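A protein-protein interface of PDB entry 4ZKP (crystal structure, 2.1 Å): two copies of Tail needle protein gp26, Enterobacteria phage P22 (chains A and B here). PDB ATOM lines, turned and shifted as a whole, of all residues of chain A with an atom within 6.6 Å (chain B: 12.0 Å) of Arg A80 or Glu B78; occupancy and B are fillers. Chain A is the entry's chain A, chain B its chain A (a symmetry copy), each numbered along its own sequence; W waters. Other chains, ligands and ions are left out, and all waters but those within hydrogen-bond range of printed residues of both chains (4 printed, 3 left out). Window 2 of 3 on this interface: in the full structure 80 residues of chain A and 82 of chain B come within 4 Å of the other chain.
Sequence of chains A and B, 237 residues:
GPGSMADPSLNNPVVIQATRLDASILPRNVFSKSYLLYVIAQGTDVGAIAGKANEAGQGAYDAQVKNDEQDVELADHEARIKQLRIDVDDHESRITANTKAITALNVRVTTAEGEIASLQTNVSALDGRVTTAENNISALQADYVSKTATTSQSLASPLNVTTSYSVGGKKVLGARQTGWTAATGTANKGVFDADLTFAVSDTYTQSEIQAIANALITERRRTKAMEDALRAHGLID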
ATOM      1  N   GLU A  73      -0.450  -8.145  17.506  1.00  0.00           N
ATOM      2  CA  GLU A  73      -1.673  -8.935  17.473  1.00  0.00           C
ATOM      3  C   GLU A  73      -1.975  -9.530  18.846  1.00  0.00           C
ATOM      4  O   GLU A  73      -3.132  -9.601  19.258  1.00  0.00           O
ATOM      5  CB  GLU A  73      -1.569 -10.044  16.428  1.00  0.00           C
ATOM      6  CG  GLU A  73      -2.826 -10.885  16.300  1.00  0.00           C
ATOM      7  CD  GLU A  73      -2.894 -11.637  14.988  1.00  0.00           C
ATOM      8  OE1 GLU A  73      -3.965 -12.200  14.680  1.00  0.00           O
ATOM      9  OE2 GLU A  73      -1.876 -11.670  14.267  1.00  0.00           O
ATOM     10  N   ALA A  75      -1.188  -8.235  21.711  1.00  0.00           N
ATOM     11  CA  ALA A  75      -1.677  -7.142  22.543  1.00  0.00           C
ATOM     12  C   ALA A  75      -3.140  -6.839  22.233  1.00  0.00           C
ATOM     13  O   ALA A  75      -3.908  -6.466  23.120  1.00  0.00           O
ATOM     14  CB  ALA A  75      -0.823  -5.899  22.345  1.00  0.00           C
ATOM     15  N   ASP A  76      -3.522  -7.003  20.971  1.00  0.00           N
ATOM     16  CA  ASP A  76      -4.896  -6.759  20.548  1.00  0.00           C
ATOM     17  C   ASP A  76      -5.822  -7.860  21.054  1.00  0.00           C
ATOM     18  O   ASP A  76      -6.933  -7.589  21.508  1.00  0.00           O
ATOM     19  CB  ASP A  76      -4.980  -6.661  19.025  1.00  0.00           C
ATOM     20  CG  ASP A  76      -6.409  -6.573  18.526  1.00  0.00           C
ATOM     21  OD1 ASP A  76      -7.137  -5.658  18.966  1.00  0.00           O
ATOM     22  OD2 ASP A  76      -6.805  -7.418  17.698  1.00  0.00           O
ATOM     23  N   HIS A  77      -5.356  -9.102  20.967  1.00  0.00           N
ATOM     24  CA  HIS A  77      -6.099 -10.240  21.493  1.00  0.00           C
ATOM     25  C   HIS A  77      -6.276 -10.123  23.002  1.00  0.00           C
ATOM     26  O   HIS A  77      -7.343 -10.420  23.536  1.00  0.00           O
ATOM     27  CB  HIS A  77      -5.387 -11.549  21.148  1.00  0.00           C
ATOM     28  CG  HIS A  77      -5.557 -11.974  19.722  1.00  0.00           C
ATOM     29  ND1 HIS A  77      -5.188 -13.221  19.270  1.00  0.00           N
ATOM     30  CD2 HIS A  77      -6.056 -11.316  18.650  1.00  0.00           C
ATOM     31  CE1 HIS A  77      -5.452 -13.315  17.978  1.00  0.00           C
ATOM     32  NE2 HIS A  77      -5.979 -12.171  17.577  1.00  0.00           N
ATOM     33  N   GLU A  78      -5.222  -9.681  23.682  1.00  0.00           N
ATOM     34  CA  GLU A  78      -5.226  -9.568  25.135  1.00  0.00           C
ATOM     35  C   GLU A  78      -6.268  -8.560  25.610  1.00  0.00           C
ATOM     36  O   GLU A  78      -6.966  -8.790  26.598  1.00  0.00           O
ATOM     37  CB  GLU A  78      -3.837  -9.164  25.636  1.00  0.00           C
ATOM     38  CG  GLU A  78      -3.754  -8.882  27.128  1.00  0.00           C
ATOM     39  CD  GLU A  78      -4.123 -10.085  27.969  1.00  0.00           C
ATOM     40  OE1 GLU A  78      -4.915  -9.927  28.923  1.00  0.00           O
ATOM     41  OE2 GLU A  78      -3.604 -11.187  27.692  1.00  0.00           O
ATOM     42  N   ALA A  79      -6.374  -7.446  24.894  1.00  0.00           N
ATOM     43  CA  ALA A  79      -7.314  -6.391  25.252  1.00  0.00           C
ATOM     44  C   ALA A  79      -8.754  -6.824  24.996  1.00  0.00           C
ATOM     45  O   ALA A  79      -9.655  -6.502  25.769  1.00  0.00           O
ATOM     46  CB  ALA A  79      -6.998  -5.117  24.480  1.00  0.00           C
ATOM     47  N   ARG A  80      -8.963  -7.554  23.906  1.00  0.00           N
ATOM     48  CA  ARG A  80     -10.298  -7.995  23.521  1.00  0.00           C
ATOM     49  C   ARG A  80     -10.789  -9.142  24.399  1.00  0.00           C
ATOM     50  O   ARG A  80     -11.987  -9.273  24.646  1.00  0.00           O
ATOM     51  CB  ARG A  80     -10.316  -8.409  22.050  1.00  0.00           C
ATOM     52  CG  ARG A  80     -10.243  -7.235  21.084  1.00  0.00           C
ATOM     53  CD  ARG A  80      -9.695  -7.657  19.731  1.00  0.00           C
ATOM     54  NE  ARG A  80     -10.616  -8.530  19.009  1.00  0.00           N
ATOM     55  CZ  ARG A  80     -10.276  -9.251  17.945  1.00  0.00           C
ATOM     56  NH1 ARG A  80      -9.035  -9.205  17.482  1.00  0.00           N
ATOM     57  NH2 ARG A  80     -11.176 -10.018  17.346  1.00  0.00           N
ATOM     58  N   ILE A  81      -9.860  -9.970  24.869  1.00  0.00           N
ATOM     59  CA  ILE A  81     -10.207 -11.063  25.769  1.00  0.00           C
ATOM     60  C   ILE A  81     -10.611 -10.483  27.120  1.00  0.00           C
ATOM     61  O   ILE A  81     -11.565 -10.949  27.747  1.00  0.00           O
ATOM     62  CB  ILE A  81      -9.044 -12.067  25.912  1.00  0.00           C
ATOM     63  CG1 ILE A  81      -8.920 -12.923  24.650  1.00  0.00           C
ATOM     64  CG2 ILE A  81      -9.249 -12.963  27.119  1.00  0.00           C
ATOM     65  CD1 ILE A  81      -7.593 -13.646  24.531  1.00  0.00           C
ATOM     66  N   LYS A  82      -9.884  -9.456  27.556  1.00  0.00           N
ATOM     67  CA  LYS A  82     -10.198  -8.758  28.800  1.00  0.00           C
ATOM     68  C   LYS A  82     -11.609  -8.181  28.788  1.00  0.00           C
ATOM     69  O   LYS A  82     -12.327  -8.264  29.781  1.00  0.00           O
ATOM     70  CB  LYS A  82      -9.190  -7.634  29.058  1.00  0.00           C
ATOM     71  CG  LYS A  82      -7.884  -8.078  29.693  1.00  0.00           C
ATOM     72  CD  LYS A  82      -7.254  -6.935  30.477  1.00  0.00           C
ATOM     73  CE  LYS A  82      -5.955  -7.356  31.143  1.00  0.00           C
ATOM     74  NZ  LYS A  82      -4.813  -7.360  30.189  1.00  0.00           N
ATOM     75  N   GLN A  83     -12.003  -7.606  27.656  1.00  0.00           N
ATOM     76  CA  GLN A  83     -13.304  -6.957  27.551  1.00  0.00           C
ATOM     77  C   GLN A  83     -14.419  -7.993  27.461  1.00  0.00           C
ATOM     78  O   GLN A  83     -15.500  -7.802  28.018  1.00  0.00           O
ATOM     79  CB  GLN A  83     -13.347  -6.028  26.338  1.00  0.00           C
ATOM     80  CG  GLN A  83     -14.597  -5.168  26.264  1.00  0.00           C
ATOM     81  CD  GLN A  83     -14.763  -4.282  27.484  1.00  0.00           C
ATOM     82  OE1 GLN A  83     -13.997  -3.342  27.690  1.00  0.00           O
ATOM     83  NE2 GLN A  83     -15.766  -4.582  28.301  1.00  0.00           N
ATOM     84  N   LEU A  84     -14.149  -9.085  26.752  1.00  0.00           N
ATOM     85  CA  LEU A  84     -15.066 -10.217  26.699  1.00  0.00           C
ATOM     86  C   LEU A  84     -15.308 -10.769  28.097  1.00  0.00           C
ATOM     87  O   LEU A  84     -16.441 -11.069  28.471  1.00  0.00           O
ATOM     88  CB  LEU A  84     -14.517 -11.312  25.785  1.00  0.00           C
ATOM     89  CG  LEU A  84     -14.694 -11.114  24.280  1.00  0.00           C
ATOM     90  CD1 LEU A  84     -14.072 -12.270  23.519  1.00  0.00           C
ATOM     91  CD2 LEU A  84     -16.164 -10.977  23.931  1.00  0.00           C
ATOM     92  N   ARG A  85     -14.228 -10.899  28.861  1.00  0.00           N
ATOM     93  CA  ARG A  85     -14.292 -11.422  30.221  1.00  0.00           C
ATOM     94  C   ARG A  85     -15.142 -10.513  31.107  1.00  0.00           C
ATOM     95  O   ARG A  85     -15.918 -10.988  31.933  1.00  0.00           O
ATOM     96  CB  ARG A  85     -12.881 -11.567  30.798  1.00  0.00           C
ATOM     97  CG  ARG A  85     -12.793 -12.278  32.142  1.00  0.00           C
ATOM     98  CD  ARG A  85     -13.101 -13.763  32.021  1.00  0.00           C
ATOM     99  NE  ARG A  85     -14.524 -14.057  32.159  1.00  0.00           N
ATOM    100  CZ  ARG A  85     -15.056 -15.261  31.971  1.00  0.00           C
ATOM    101  NH1 ARG A  85     -14.285 -16.283  31.628  1.00  0.00           N
ATOM    102  NH2 ARG A  85     -16.360 -15.441  32.122  1.00  0.00           N
ATOM    103  N   GLU B  69       3.715 -21.448  12.755  1.00  0.00           N
ATOM    104  CA  GLU B  69       2.764 -22.154  13.605  1.00  0.00           C
ATOM    105  C   GLU B  69       2.187 -21.214  14.662  1.00  0.00           C
ATOM    106  O   GLU B  69       1.056 -21.400  15.112  1.00  0.00           O
ATOM    107  CB  GLU B  69       3.419 -23.386  14.240  1.00  0.00           C
ATOM    108  CG  GLU B  69       4.512 -23.102  15.250  1.00  0.00           C
ATOM    109  CD  GLU B  69       4.825 -24.308  16.116  1.00  0.00           C
ATOM    110  OE1 GLU B  69       4.823 -25.438  15.582  1.00  0.00           O
ATOM    111  OE2 GLU B  69       5.078 -24.127  17.325  1.00  0.00           O
ATOM    112  N   GLN B  70       2.963 -20.212  15.064  1.00  0.00           N
ATOM    113  CA  GLN B  70       2.450 -19.177  15.957  1.00  0.00           C
ATOM    114  C   GLN B  70       1.403 -18.346  15.222  1.00  0.00           C
ATOM    115  O   GLN B  70       0.384 -17.964  15.794  1.00  0.00           O
ATOM    116  CB  GLN B  70       3.574 -18.276  16.475  1.00  0.00           C
ATOM    117  CG  GLN B  70       4.324 -18.828  17.677  1.00  0.00           C
ATOM    118  CD  GLN B  70       5.579 -18.036  17.989  1.00  0.00           C
ATOM    119  OE1 GLN B  70       6.004 -17.192  17.201  1.00  0.00           O
ATOM    120  NE2 GLN B  70       6.170 -18.295  19.149  1.00  0.00           N
ATOM    121  N   ASP B  71       1.674 -18.069  13.950  1.00  0.00           N
ATOM    122  CA  ASP B  71       0.736 -17.362  13.084  1.00  0.00           C
ATOM    123  C   ASP B  71      -0.569 -18.138  12.932  1.00  0.00           C
ATOM    124  O   ASP B  71      -1.651 -17.552  12.918  1.00  0.00           O
ATOM    125  CB  ASP B  71       1.360 -17.107  11.711  1.00  0.00           C
ATOM    126  CG  ASP B  71       2.301 -15.915  11.711  1.00  0.00           C
ATOM    127  OD1 ASP B  71       2.421 -15.250  12.761  1.00  0.00           O
ATOM    128  OD2 ASP B  71       2.922 -15.648  10.661  1.00  0.00           O
ATOM    129  N   VAL B  72      -0.455 -19.457  12.808  1.00  0.00           N
ATOM    130  CA  VAL B  72      -1.619 -20.324  12.660  1.00  0.00           C
ATOM    131  C   VAL B  72      -2.503 -20.219  13.897  1.00  0.00           C
ATOM    132  O   VAL B  72      -3.726 -20.123  13.793  1.00  0.00           O
ATOM    133  CB  VAL B  72      -1.195 -21.785  12.408  1.00  0.00           C
ATOM    134  CG1 VAL B  72      -2.380 -22.726  12.570  1.00  0.00           C
ATOM    135  CG2 VAL B  72      -0.587 -21.929  11.019  1.00  0.00           C
ATOM    136  N   GLU B  73      -1.874 -20.227  15.067  1.00  0.00           N
ATOM    137  CA  GLU B  73      -2.601 -20.137  16.326  1.00  0.00           C
ATOM    138  C   GLU B  73      -3.236 -18.759  16.493  1.00  0.00           C
ATOM    139  O   GLU B  73      -4.351 -18.639  16.998  1.00  0.00           O
ATOM    140  CB  GLU B  73      -1.676 -20.439  17.504  1.00  0.00           C
ATOM    141  CG  GLU B  73      -2.372 -20.411  18.853  1.00  0.00           C
ATOM    142  CD  GLU B  73      -1.600 -21.152  19.924  1.00  0.00           C
ATOM    143  OE1 GLU B  73      -2.162 -21.371  21.017  1.00  0.00           O
ATOM    144  OE2 GLU B  73      -0.431 -21.510  19.675  1.00  0.00           O
ATOM    145  N   LEU B  74      -2.514 -17.726  16.070  1.00  0.00           N
ATOM    146  CA  LEU B  74      -3.015 -16.358  16.127  1.00  0.00           C
ATOM    147  C   LEU B  74      -4.270 -16.196  15.276  1.00  0.00           C
ATOM    148  O   LEU B  74      -5.215 -15.514  15.673  1.00  0.00           O
ATOM    149  CB  LEU B  74      -1.939 -15.372  15.671  1.00  0.00           C
ATOM    150  CG  LEU B  74      -0.853 -15.034  16.691  1.00  0.00           C
ATOM    151  CD1 LEU B  74       0.217 -14.162  16.062  1.00  0.00           C
ATOM    152  CD2 LEU B  74      -1.458 -14.352  17.899  1.00  0.00           C
ATOM    153  N   ALA B  75      -4.269 -16.825  14.105  1.00  0.00           N
ATOM    154  CA  ALA B  75      -5.417 -16.781  13.207  1.00  0.00           C
ATOM    155  C   ALA B  75      -6.606 -17.520  13.813  1.00  0.00           C
ATOM    156  O   ALA B  75      -7.757 -17.136  13.609  1.00  0.00           O
ATOM    157  CB  ALA B  75      -5.056 -17.373  11.853  1.00  0.00           C
ATOM    158  N   ASP B  76      -6.322 -18.583  14.560  1.00  0.00           N
ATOM    159  CA  ASP B  76      -7.368 -19.368  15.205  1.00  0.00           C
ATOM    160  C   ASP B  76      -7.971 -18.606  16.380  1.00  0.00           C
ATOM    161  O   ASP B  76      -9.186 -18.609  16.575  1.00  0.00           O
ATOM    162  CB  ASP B  76      -6.815 -20.712  15.679  1.00  0.00           C
ATOM    163  CG  ASP B  76      -7.820 -21.495  16.501  1.00  0.00           C
ATOM    164  OD1 ASP B  76      -8.935 -21.746  15.997  1.00  0.00           O
ATOM    165  OD2 ASP B  76      -7.497 -21.858  17.650  1.00  0.00           O
ATOM    166  N   HIS B  77      -7.111 -17.956  17.158  1.00  0.00           N
ATOM    167  CA  HIS B  77      -7.559 -17.117  18.262  1.00  0.00           C
ATOM    168  C   HIS B  77      -8.397 -15.950  17.754  1.00  0.00           C
ATOM    169  O   HIS B  77      -9.411 -15.595  18.353  1.00  0.00           O
ATOM    170  CB  HIS B  77      -6.360 -16.595  19.057  1.00  0.00           C
ATOM    171  CG  HIS B  77      -5.738 -17.616  19.957  1.00  0.00           C
ATOM    172  ND1 HIS B  77      -4.799 -17.293  20.912  1.00  0.00           N
ATOM    173  CD2 HIS B  77      -5.921 -18.954  20.046  1.00  0.00           C
ATOM    174  CE1 HIS B  77      -4.430 -18.388  21.552  1.00  0.00           C
ATOM    175  NE2 HIS B  77      -5.095 -19.411  21.046  1.00  0.00           N
ATOM    176  N   GLU B  78      -7.968 -15.363  16.642  1.00  0.00           N
ATOM    177  CA  GLU B  78      -8.637 -14.202  16.066  1.00  0.00           C
ATOM    178  C   GLU B  78     -10.061 -14.541  15.636  1.00  0.00           C
ATOM    179  O   GLU B  78     -10.986 -13.754  15.842  1.00  0.00           O
ATOM    180  CB  GLU B  78      -7.839 -13.670  14.874  1.00  0.00           C
ATOM    181  CG  GLU B  78      -8.512 -12.542  14.108  1.00  0.00           C
ATOM    182  CD  GLU B  78      -8.760 -11.321  14.970  1.00  0.00           C
ATOM    183  OE1 GLU B  78      -9.885 -10.779  14.926  1.00  0.00           O
ATOM    184  OE2 GLU B  78      -7.823 -10.889  15.674  1.00  0.00           O
ATOM    185  N   ALA B  79     -10.230 -15.717  15.045  1.00  0.00           N
ATOM    186  CA  ALA B  79     -11.535 -16.153  14.564  1.00  0.00           C
ATOM    187  C   ALA B  79     -12.472 -16.476  15.723  1.00  0.00           C
ATOM    188  O   ALA B  79     -13.667 -16.192  15.667  1.00  0.00           O
ATOM    189  CB  ALA B  79     -11.386 -17.362  13.651  1.00  0.00           C
ATOM    190  N   ARG B  80     -11.920 -17.075  16.775  1.00  0.00           N
ATOM    191  CA  ARG B  80     -12.711 -17.479  17.930  1.00  0.00           C
ATOM    192  C   ARG B  80     -13.096 -16.283  18.797  1.00  0.00           C
ATOM    193  O   ARG B  80     -14.154 -16.281  19.427  1.00  0.00           O
ATOM    194  CB  ARG B  80     -11.947 -18.510  18.761  1.00  0.00           C
ATOM    195  CG  ARG B  80     -11.881 -19.886  18.115  1.00  0.00           C
ATOM    196  CD  ARG B  80     -10.694 -20.687  18.625  1.00  0.00           C
ATOM    197  NE  ARG B  80     -10.844 -21.065  20.027  1.00  0.00           N
ATOM    198  CZ  ARG B  80      -9.850 -21.521  20.784  1.00  0.00           C
ATOM    199  NH1 ARG B  80      -8.634 -21.653  20.272  1.00  0.00           N
ATOM    200  NH2 ARG B  80     -10.072 -21.846  22.050  1.00  0.00           N
ATOM    201  N   ILE B  81     -12.237 -15.268  18.826  1.00  0.00           N
ATOM    202  CA  ILE B  81     -12.531 -14.049  19.568  1.00  0.00           C
ATOM    203  C   ILE B  81     -13.652 -13.296  18.861  1.00  0.00           C
ATOM    204  O   ILE B  81     -14.553 -12.755  19.505  1.00  0.00           O
ATOM    205  CB  ILE B  81     -11.273 -13.168  19.728  1.00  0.00           C
ATOM    206  CG1 ILE B  81     -10.327 -13.772  20.768  1.00  0.00           C
ATOM    207  CG2 ILE B  81     -11.651 -11.758  20.140  1.00  0.00           C
ATOM    208  CD1 ILE B  81      -8.919 -13.214  20.708  1.00  0.00           C
ATOM    209  N   LYS B  82     -13.595 -13.279  17.530  1.00  0.00           N
ATOM    210  CA  LYS B  82     -14.636 -12.653  16.719  1.00  0.00           C
ATOM    211  C   LYS B  82     -16.006 -13.268  16.981  1.00  0.00           C
ATOM    212  O   LYS B  82     -17.003 -12.556  17.078  1.00  0.00           O
ATOM    213  CB  LYS B  82     -14.302 -12.769  15.228  1.00  0.00           C
ATOM    214  CG  LYS B  82     -13.333 -11.722  14.706  1.00  0.00           C
ATOM    215  CD  LYS B  82     -13.547 -11.491  13.216  1.00  0.00           C
ATOM    216  CE  LYS B  82     -12.607 -10.431  12.669  1.00  0.00           C
ATOM    217  NZ  LYS B  82     -11.244 -10.972  12.412  1.00  0.00           N
ATOM    218  N   GLN B  83     -16.047 -14.591  17.103  1.00  0.00           N
ATOM    219  CA  GLN B  83     -17.311 -15.295  17.284  1.00  0.00           C
ATOM    220  C   GLN B  83     -17.837 -15.106  18.701  1.00  0.00           C
ATOM    221  O   GLN B  83     -19.043 -14.977  18.912  1.00  0.00           O
ATOM    222  CB  GLN B  83     -17.148 -16.782  16.973  1.00  0.00           C
ATOM    223  CG  GLN B  83     -18.458 -17.552  16.949  1.00  0.00           C
ATOM    224  CD  GLN B  83     -19.431 -17.008  15.921  1.00  0.00           C
ATOM    225  OE1 GLN B  83     -19.212 -17.131  14.717  1.00  0.00           O
ATOM    226  NE2 GLN B  83     -20.513 -16.400  16.394  1.00  0.00           N
ATOM    227  N   LEU B  84     -16.925 -15.096  19.669  1.00  0.00           N
ATOM    228  CA  LEU B  84     -17.270 -14.785  21.050  1.00  0.00           C
ATOM    229  C   LEU B  84     -17.880 -13.393  21.143  1.00  0.00           C
ATOM    230  O   LEU B  84     -18.879 -13.186  21.832  1.00  0.00           O
ATOM    231  CB  LEU B  84     -16.036 -14.882  21.948  1.00  0.00           C
ATOM    232  CG  LEU B  84     -15.603 -16.282  22.384  1.00  0.00           C
ATOM    233  CD1 LEU B  84     -14.354 -16.205  23.241  1.00  0.00           C
ATOM    234  CD2 LEU B  84     -16.724 -16.973  23.137  1.00  0.00           C
ATOM    235  N   ARG B  85     -17.266 -12.444  20.444  1.00  0.00           N
ATOM    236  CA  ARG B  85     -17.722 -11.060  20.436  1.00  0.00           C
ATOM    237  C   ARG B  85     -19.129 -10.961  19.848  1.00  0.00           C
ATOM    238  O   ARG B  85     -19.964 -10.207  20.343  1.00  0.00           O
ATOM    239  CB  ARG B  85     -16.746 -10.186  19.643  1.00  0.00           C
ATOM    240  CG  ARG B  85     -17.004  -8.687  19.712  1.00  0.00           C
ATOM    241  CD  ARG B  85     -16.688  -8.120  21.088  1.00  0.00           C
ATOM    242  NE  ARG B  85     -17.829  -8.179  21.998  1.00  0.00           N
ATOM    243  CZ  ARG B  85     -17.769  -7.857  23.286  1.00  0.00           C
ATOM    244  NH1 ARG B  85     -16.622  -7.462  23.822  1.00  0.00           N
ATOM    245  NH2 ARG B  85     -18.856  -7.934  24.040  1.00  0.00           N
ATOM    246  N   ILE B  86     -19.377 -11.727  18.791  1.00  0.00           N
ATOM    247  CA  ILE B  86     -20.693 -11.788  18.164  1.00  0.00           C
ATOM    248  C   ILE B  86     -21.730 -12.325  19.144  1.00  0.00           C
ATOM    249  O   ILE B  86     -22.810 -11.754  19.297  1.00  0.00           O
ATOM    250  CB  ILE B  86     -20.661 -12.651  16.886  1.00  0.00           C
ATOM    251  CG1 ILE B  86     -19.860 -11.953  15.786  1.00  0.00           C
ATOM    252  CG2 ILE B  86     -22.072 -12.965  16.410  1.00  0.00           C
ATOM    253  CD1 ILE B  86     -19.760 -12.751  14.505  1.00  0.00           C
ATOM    254  N   ASP B  87     -21.387 -13.424  19.809  1.00  0.00           N
ATOM    255  CA  ASP B  87     -22.298 -14.090  20.731  1.00  0.00           C
ATOM    256  C   ASP B  87     -22.622 -13.221  21.942  1.00  0.00           C
ATOM    257  O   ASP B  87     -23.770 -13.155  22.379  1.00  0.00           O
ATOM    258  CB  ASP B  87     -21.708 -15.421  21.192  1.00  0.00           C
ATOM    259  CG  ASP B  87     -21.500 -16.394  20.049  1.00  0.00           C
ATOM    260  OD1 ASP B  87     -22.105 -16.190  18.976  1.00  0.00           O
ATOM    261  OD2 ASP B  87     -20.729 -17.360  20.223  1.00  0.00           O
ATOM    262  N   VAL B  88     -21.606 -12.556  22.483  1.00  0.00           N
ATOM    263  CA  VAL B  88     -21.785 -11.750  23.683  1.00  0.00           C
ATOM    264  C   VAL B  88     -22.583 -10.486  23.356  1.00  0.00           C
ATOM    265  O   VAL B  88     -23.422 -10.051  24.145  1.00  0.00           O
ATOM    266  CB  VAL B  88     -20.427 -11.402  24.321  1.00  0.00           C
ATOM    267  CG1 VAL B  88     -20.596 -10.363  25.407  1.00  0.00           C
ATOM    268  CG2 VAL B  88     -19.771 -12.656  24.882  1.00  0.00           C
ATOM    269  N   ASP B  89     -22.337  -9.915  22.180  1.00  0.00           N
ATOM    270  CA  ASP B  89     -23.116  -8.772  21.712  1.00  0.00           C
ATOM    271  C   ASP B  89     -24.571  -9.173  21.496  1.00  0.00           C
ATOM    272  O   ASP B  89     -25.483  -8.368  21.681  1.00  0.00           O
ATOM    273  CB  ASP B  89     -22.525  -8.200  20.422  1.00  0.00           C
ATOM    274  CG  ASP B  89     -21.222  -7.461  20.655  1.00  0.00           C
ATOM    275  OD1 ASP B  89     -20.886  -7.206  21.830  1.00  0.00           O
ATOM    276  OD2 ASP B  89     -20.535  -7.138  19.664  1.00  0.00           O
HETATM  277  O   HOH W   1     -13.890  -7.805  23.296  1.00  0.00           O
HETATM  278  O   HOH W   2      -0.135 -13.642  12.504  1.00  0.00           O
HETATM  279  O   HOH W   3      -3.761 -14.812  20.903  1.00  0.00           O
HETATM  280  O   HOH W   4      -9.530  -8.026  14.626  1.00  0.00           O
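OE2 of Glu B78 lies within hydrogen-bond range of NE2 of His A77 (2.9 Å). The guanidinium group (NH1) of Arg A80 lies within salt-bridge range of the side-chain carboxylate (OE2) of Glu B78, 2.8 Å away.
The guanidinium group (NH2) of Arg B85 is in salt-bridge range of the side-chain carboxylate (OD1) of Asp B89 (3.1 Å). The side-chain carboxylate (OE1) of Glu B78 lies within salt-bridge range of the side-chain amino group (NZ) of Lys B82. OD2 of Asp A76 lies within salt-bridge range of NH1 of Arg A80 (2.9 Å).
Leu B74 touches Glu A73. His A77 touches Leu B74. His B77 touches His A77. His A77 touches Ile B81. NH2 of Arg A80 touches CG2 of Ile B81, at 3.3 Å. NH2 of Arg A80 touches CG of Lys B82, at 3.8 Å. Ile A81 touches Ile B81. Gln A83 touches Arg B85. Leu B84 touches Leu A84 (CB to CD1, 3.6 Å). Arg B85 touches Leu A84.
Arg A80 touches just these residues of chain B: Glu B78, Ile B81 and Lys B82. Glu B78 touches two residues of chain A. No residue of chain B comes within 4 Å of Asp A76. Of chain B, only Leu B74, His B77, Glu B78 and Ile B81 come within 4 Å of His A77. No residue of chain B comes within 4 Å of Glu A78. Leu A84 touches two residues of chain B. Of the printed residues of chain A, Ile B81 touches His A77, Arg A80 and Ile A81. Printed residues of chain A within 4 Å of Leu B84: Leu A84. Of the printed residues of chain A, His B77 touches His A77 (3.6 Å). The nearest residue of chain B that does not touch Arg A80 is Arg B85 (5.0 Å). The nearest printed residue of chain A that does not touch Glu B78 is Asp A76 (4.1 Å).
Hydrophobic or aromatic side chains of chain B within 4 Å of the printed part of chain A: Leu B74, His B77, Ile B81 and Leu B84. Of the 12 printed residues of chain A, 6 touch a printed residue of chain B. Hydrophobic or aromatic side chains of chain A that line the printed part of chain B: His A77, Ile A81 and Leu A84. Among the printed residues, Asp or Glu carboxylates within 4 Å of a Lys or Arg side-chain nitrogen of the other chain: Arg A80 with Glu B78 (2.8 Å).
Arg A80 touches Glu B78, but with the chains exchanged Glu A78 does not touch Arg B80 (11.4 Å). Arg A80 touches Ile B81, but with the chains exchanged Ile A81 does not touch Arg B80 (7.9 Å). Arg A80 touches Lys B82, but with the chains exchanged Lys A82 does not touch Arg B80 (11.4 Å). Ile B81 touches its own counterpart, Ile A81.
Water W3 lies within hydrogen-bond range of a ring nitrogen (ND1) of His A77 (2.7 Å) and a ring nitrogen (ND1) of His B77 (2.7 Å). Water W1 lies within hydrogen-bond range of O of Arg A80 (2.8 Å) and NH1 of Arg B85 (2.8 Å). Water W4 lies within hydrogen-bond range of OE1 of Glu B78 (2.8 Å) and NH1 of Arg A80 (3.1 Å). Water W2 bridges the side-chain carboxylate (OD1) of Asp B71 and the side-chain carboxylate (OE2) of Glu A73.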
